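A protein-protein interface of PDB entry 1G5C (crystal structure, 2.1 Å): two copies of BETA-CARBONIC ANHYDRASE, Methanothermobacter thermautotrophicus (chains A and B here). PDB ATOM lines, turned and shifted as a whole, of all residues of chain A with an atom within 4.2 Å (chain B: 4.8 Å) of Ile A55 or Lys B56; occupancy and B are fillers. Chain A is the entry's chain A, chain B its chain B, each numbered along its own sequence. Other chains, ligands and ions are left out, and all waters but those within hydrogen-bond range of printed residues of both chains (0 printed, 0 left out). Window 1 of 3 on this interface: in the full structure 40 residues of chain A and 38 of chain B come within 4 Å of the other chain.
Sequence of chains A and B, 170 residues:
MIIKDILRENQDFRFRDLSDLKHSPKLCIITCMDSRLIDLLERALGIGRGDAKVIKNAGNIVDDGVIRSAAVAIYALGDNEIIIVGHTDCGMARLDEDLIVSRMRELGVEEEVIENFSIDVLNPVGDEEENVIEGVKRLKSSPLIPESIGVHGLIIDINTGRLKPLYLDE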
ATOM      1  N   CYS A  28      21.281  18.048  -7.954  1.00  0.00           N
ATOM      2  CA  CYS A  28      20.245  17.261  -8.618  1.00  0.00           C
ATOM      3  C   CYS A  28      20.769  17.028 -10.023  1.00  0.00           C
ATOM      4  O   CYS A  28      21.125  17.985 -10.729  1.00  0.00           O
ATOM      5  CB  CYS A  28      18.909  17.987  -8.708  1.00  0.00           C
ATOM      6  SG  CYS A  28      17.715  16.996  -9.677  1.00  0.00           S
ATOM      7  N   ILE A  29      20.838  15.761 -10.423  1.00  0.00           N
ATOM      8  CA  ILE A  29      21.320  15.393 -11.749  1.00  0.00           C
ATOM      9  C   ILE A  29      20.124  14.925 -12.584  1.00  0.00           C
ATOM     10  O   ILE A  29      19.288  14.128 -12.120  1.00  0.00           O
ATOM     11  CB  ILE A  29      22.340  14.205 -11.695  1.00  0.00           C
ATOM     12  CG1 ILE A  29      23.494  14.491 -10.726  1.00  0.00           C
ATOM     13  CG2 ILE A  29      22.874  13.923 -13.089  1.00  0.00           C
ATOM     14  CD1 ILE A  29      24.475  15.547 -11.202  1.00  0.00           C
ATOM     15  N   ILE A  30      20.035  15.420 -13.811  1.00  0.00           N
ATOM     16  CA  ILE A  30      18.978  15.002 -14.722  1.00  0.00           C
ATOM     17  C   ILE A  30      19.692  14.317 -15.898  1.00  0.00           C
ATOM     18  O   ILE A  30      20.546  14.925 -16.556  1.00  0.00           O
ATOM     19  CB  ILE A  30      18.155  16.212 -15.234  1.00  0.00           C
ATOM     20  CG1 ILE A  30      17.383  16.838 -14.069  1.00  0.00           C
ATOM     21  CG2 ILE A  30      17.172  15.761 -16.308  1.00  0.00           C
ATOM     22  CD1 ILE A  30      16.742  18.186 -14.372  1.00  0.00           C
ATOM     23  N   THR A  31      19.370  13.051 -16.147  1.00  0.00           N
ATOM     24  CA  THR A  31      20.011  12.344 -17.242  1.00  0.00           C
ATOM     25  C   THR A  31      19.100  11.306 -17.902  1.00  0.00           C
ATOM     26  O   THR A  31      17.876  11.293 -17.669  1.00  0.00           O
ATOM     27  CB  THR A  31      21.364  11.716 -16.771  1.00  0.00           C
ATOM     28  OG1 THR A  31      22.109  11.259 -17.918  1.00  0.00           O
ATOM     29  CG2 THR A  31      21.119  10.553 -15.769  1.00  0.00           C
ATOM     30  N   VAL A  54      18.737  12.013  -8.193  1.00  0.00           N
ATOM     31  CA  VAL A  54      18.871  11.690  -9.615  1.00  0.00           C
ATOM     32  C   VAL A  54      17.549  11.448 -10.343  1.00  0.00           C
ATOM     33  O   VAL A  54      16.754  10.597  -9.948  1.00  0.00           O
ATOM     34  CB  VAL A  54      19.795  10.436  -9.800  1.00  0.00           C
ATOM     35  CG1 VAL A  54      20.051  10.158 -11.290  1.00  0.00           C
ATOM     36  CG2 VAL A  54      21.122  10.661  -9.096  1.00  0.00           C
ATOM     37  N   ILE A  55      17.329  12.210 -11.413  1.00  0.00           N
ATOM     38  CA  ILE A  55      16.124  12.073 -12.230  1.00  0.00           C
ATOM     39  C   ILE A  55      16.540  11.466 -13.566  1.00  0.00           C
ATOM     40  O   ILE A  55      17.554  11.868 -14.146  1.00  0.00           O
ATOM     41  CB  ILE A  55      15.478  13.449 -12.468  1.00  0.00           C
ATOM     42  CG1 ILE A  55      15.080  14.057 -11.119  1.00  0.00           C
ATOM     43  CG2 ILE A  55      14.254  13.316 -13.392  1.00  0.00           C
ATOM     44  CD1 ILE A  55      14.686  15.552 -11.179  1.00  0.00           C
ATOM     45  N   LYS A  56      15.773  10.499 -14.063  1.00  0.00           N
ATOM     46  CA  LYS A  56      16.100   9.854 -15.335  1.00  0.00           C
ATOM     47  C   LYS A  56      14.855   9.498 -16.136  1.00  0.00           C
ATOM     48  O   LYS A  56      13.878   8.980 -15.592  1.00  0.00           O
ATOM     49  CB  LYS A  56      16.891   8.540 -15.116  1.00  0.00           C
ATOM     50  CG  LYS A  56      18.288   8.681 -14.509  1.00  0.00           C
ATOM     51  CD  LYS A  56      18.978   7.295 -14.394  1.00  0.00           C
ATOM     52  CE  LYS A  56      20.417   7.390 -13.909  1.00  0.00           C
ATOM     53  NZ  LYS A  56      21.133   6.067 -14.094  1.00  0.00           N
ATOM     54  N   VAL A  66       9.689  16.101 -14.995  1.00  0.00           N
ATOM     55  CA  VAL A  66      11.039  16.402 -14.564  1.00  0.00           C
ATOM     56  C   VAL A  66      11.066  17.685 -13.736  1.00  0.00           C
ATOM     57  O   VAL A  66      11.706  17.743 -12.674  1.00  0.00           O
ATOM     58  CB  VAL A  66      11.976  16.538 -15.791  1.00  0.00           C
ATOM     59  CG1 VAL A  66      13.313  17.152 -15.381  1.00  0.00           C
ATOM     60  CG2 VAL A  66      12.193  15.167 -16.403  1.00  0.00           C
ATOM     61  N   SER A  69       9.742  17.083 -10.250  1.00  0.00           N
ATOM     62  CA  SER A  69      10.665  16.329  -9.410  1.00  0.00           C
ATOM     63  C   SER A  69      11.813  17.233  -8.988  1.00  0.00           C
ATOM     64  O   SER A  69      12.270  17.191  -7.842  1.00  0.00           O
ATOM     65  CB  SER A  69      11.211  15.107 -10.166  1.00  0.00           C
ATOM     66  OG  SER A  69      10.284  14.029 -10.131  1.00  0.00           O
ATOM     67  N   ALA A  70      12.287  18.062  -9.911  1.00  0.00           N
ATOM     68  CA  ALA A  70      13.372  18.983  -9.583  1.00  0.00           C
ATOM     69  C   ALA A  70      12.880  19.992  -8.535  1.00  0.00           C
ATOM     70  O   ALA A  70      13.607  20.330  -7.596  1.00  0.00           O
ATOM     71  CB  ALA A  70      13.846  19.704 -10.835  1.00  0.00           C
ATOM     72  N   THR B  31      12.455   3.713 -10.232  1.00  0.00           N
ATOM     73  CA  THR B  31      12.651   3.911  -8.804  1.00  0.00           C
ATOM     74  C   THR B  31      12.672   5.388  -8.457  1.00  0.00           C
ATOM     75  O   THR B  31      12.296   6.220  -9.298  1.00  0.00           O
ATOM     76  CB  THR B  31      13.934   3.139  -8.301  1.00  0.00           C
ATOM     77  OG1 THR B  31      13.986   3.181  -6.872  1.00  0.00           O
ATOM     78  CG2 THR B  31      15.216   3.746  -8.874  1.00  0.00           C
ATOM     79  N   CYS B  32      13.066   5.715  -7.219  1.00  0.00           N
ATOM     80  CA  CYS B  32      13.078   7.096  -6.746  1.00  0.00           C
ATOM     81  C   CYS B  32      14.388   7.850  -6.967  1.00  0.00           C
ATOM     82  O   CYS B  32      15.433   7.236  -7.144  1.00  0.00           O
ATOM     83  CB  CYS B  32      12.715   7.136  -5.251  1.00  0.00           C
ATOM     84  SG  CYS B  32      12.473   8.805  -4.585  1.00  0.00           S
ATOM     85  N   MET B  33      14.323   9.183  -6.926  1.00  0.00           N
ATOM     86  CA  MET B  33      15.518  10.024  -7.120  1.00  0.00           C
ATOM     87  C   MET B  33      16.383  10.133  -5.861  1.00  0.00           C
ATOM     88  O   MET B  33      17.472  10.707  -5.892  1.00  0.00           O
ATOM     89  CB  MET B  33      15.108  11.432  -7.569  1.00  0.00           C
ATOM     90  CG  MET B  33      14.203  12.163  -6.601  1.00  0.00           C
ATOM     91  SD  MET B  33      13.786  13.833  -7.222  1.00  0.00           S
ATOM     92  CE  MET B  33      13.314  14.623  -5.701  1.00  0.00           C
ATOM     93  N   ILE B  38      21.683   5.576  -4.689  1.00  0.00           N
ATOM     94  CA  ILE B  38      22.897   5.510  -5.522  1.00  0.00           C
ATOM     95  C   ILE B  38      23.849   4.448  -4.958  1.00  0.00           C
ATOM     96  O   ILE B  38      24.143   4.443  -3.755  1.00  0.00           O
ATOM     97  CB  ILE B  38      23.640   6.868  -5.576  1.00  0.00           C
ATOM     98  CG1 ILE B  38      22.746   7.930  -6.227  1.00  0.00           C
ATOM     99  CG2 ILE B  38      24.926   6.738  -6.417  1.00  0.00           C
ATOM    100  CD1 ILE B  38      23.308   9.337  -6.098  1.00  0.00           C
ATOM    101  N   VAL B  54      17.044   2.666 -16.673  1.00  0.00           N
ATOM    102  CA  VAL B  54      16.597   3.139 -15.375  1.00  0.00           C
ATOM    103  C   VAL B  54      15.850   4.459 -15.434  1.00  0.00           C
ATOM    104  O   VAL B  54      16.377   5.456 -15.919  1.00  0.00           O
ATOM    105  CB  VAL B  54      17.775   3.301 -14.409  1.00  0.00           C
ATOM    106  CG1 VAL B  54      17.263   3.801 -13.056  1.00  0.00           C
ATOM    107  CG2 VAL B  54      18.523   1.963 -14.273  1.00  0.00           C
ATOM    108  N   ILE B  55      14.625   4.455 -14.923  1.00  0.00           N
ATOM    109  CA  ILE B  55      13.780   5.646 -14.871  1.00  0.00           C
ATOM    110  C   ILE B  55      13.664   6.056 -13.402  1.00  0.00           C
ATOM    111  O   ILE B  55      13.374   5.216 -12.541  1.00  0.00           O
ATOM    112  CB  ILE B  55      12.358   5.335 -15.422  1.00  0.00           C
ATOM    113  CG1 ILE B  55      12.444   4.978 -16.913  1.00  0.00           C
ATOM    114  CG2 ILE B  55      11.449   6.523 -15.204  1.00  0.00           C
ATOM    115  CD1 ILE B  55      11.198   4.227 -17.447  1.00  0.00           C
ATOM    116  N   LYS B  56      13.865   7.338 -13.113  1.00  0.00           N
ATOM    117  CA  LYS B  56      13.814   7.826 -11.737  1.00  0.00           C
ATOM    118  C   LYS B  56      13.086   9.158 -11.631  1.00  0.00           C
ATOM    119  O   LYS B  56      13.277  10.035 -12.466  1.00  0.00           O
ATOM    120  CB  LYS B  56      15.240   8.040 -11.196  1.00  0.00           C
ATOM    121  CG  LYS B  56      16.036   6.773 -10.925  1.00  0.00           C
ATOM    122  CD  LYS B  56      17.364   7.113 -10.229  1.00  0.00           C
ATOM    123  CE  LYS B  56      18.183   5.888  -9.842  1.00  0.00           C
ATOM    124  NZ  LYS B  56      19.378   6.283  -9.009  1.00  0.00           N
ATOM    125  N   ASN B  57      12.245   9.303 -10.607  1.00  0.00           N
ATOM    126  CA  ASN B  57      11.562  10.570 -10.371  1.00  0.00           C
ATOM    127  C   ASN B  57      11.257  10.653  -8.873  1.00  0.00           C
ATOM    128  O   ASN B  57      11.605   9.744  -8.111  1.00  0.00           O
ATOM    129  CB  ASN B  57      10.284  10.694 -11.219  1.00  0.00           C
ATOM    130  CG  ASN B  57       9.178   9.775 -10.758  1.00  0.00           C
ATOM    131  OD1 ASN B  57       9.295   9.087  -9.737  1.00  0.00           O
ATOM    132  ND2 ASN B  57       8.080   9.759 -11.509  1.00  0.00           N
ATOM    133  N   ALA B  58      10.629  11.743  -8.452  1.00  0.00           N
ATOM    134  CA  ALA B  58      10.303  11.950  -7.053  1.00  0.00           C
ATOM    135  C   ALA B  58       9.259  10.938  -6.568  1.00  0.00           C
ATOM    136  O   ALA B  58       8.090  11.010  -6.950  1.00  0.00           O
ATOM    137  CB  ALA B  58       9.791  13.362  -6.844  1.00  0.00           C
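OG of Ser A69 is in hydrogen-bond range of N of Ala B58 (2.9 Å).
N of Val A54 lies within hydrogen-bond range of O of Met B33 (2.9 Å).
The backbone carbonyl oxygen (O) of Lys A56 is in hydrogen-bond range of the backbone NH (N) of Lys B56 (3.0 Å).
O of Ser A69 lies close to SD of Met B33, 3.7 Å away.
The backbone carbonyl oxygen of Ile A29 is in hydrogen-bond range of the backbone NH of Ile A55, 2.8 Å away.
SG of Cys B32 sits close to O of Asn B57 (3.8 Å).
The backbone NH (N) of Thr A31 lies within hydrogen-bond range of the backbone carbonyl oxygen (O) of Ile A55.
The backbone carbonyl oxygen (O) of Asn B57 lies within hydrogen-bond range of the backbone NH (N) of Met B33, 3.0 Å away.
The backbone NH of Thr B31 lies within hydrogen-bond range of the backbone carbonyl oxygen of Ile B55 (2.9 Å).
The backbone carbonyl oxygen (O) of Thr B31 is in hydrogen-bond range of the backbone NH (N) of Asn B57, 3.3 Å away.
Val A54 touches Lys B56, and with the chains exchanged Lys A56 touches Val B54.
Ile A55 touches Lys B56, and with the chains exchanged Lys A56 touches Ile B55.
Lys A56 touches its own counterpart, Lys B56.
Val A54 touches Ile B38 (CG2 to CD1, 3.9 Å).
O of Val A54 touches CB of Lys B56 (3.2 Å).
O of Lys B56 touches CA of Ile A55, 3.5 Å away.
Val B54 touches Lys A56.
Lys A56 touches Ile B55.
OG of Ser A69 touches CB of Asn B57, 3.5 Å away.
Ile A55 touches just one residue of chain B: Lys B56 (3.5 Å).
Lys B56 touches just these residues of chain A: Val A54 (3.2 Å), Ile A55 (3.5 Å) and Lys A56 (3.0 Å).
Of the printed residues of chain A, Ile B55 touches Lys A56 (3.4 Å).
Of the printed residues of chain B, Val A54 touches Met B33 (2.9 Å), Ile B38 (3.9 Å) and Lys B56 (3.2 Å).
Printed residues of chain A within 4 Å of Val B54: Lys A56 (3.2 Å).
Of the printed residues of chain B, Ser A69 touches Met B33, Asn B57 and Ala B58.
Thr B31 touches none of the printed residues of chain A.
The nearest residue of chain B that does not touch Ile A55 is Met B33 (4.1 Å).
Hydrophobic or aromatic side chains of chain A that line the printed part of chain B: Val A54 and Ile A55.
Among the printed residues, 10 pairs touch across the chains.
Among the printed residues, no Asp or Glu carboxylate lies within 4 Å of a Lys or Arg side-chain nitrogen of the other chain.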
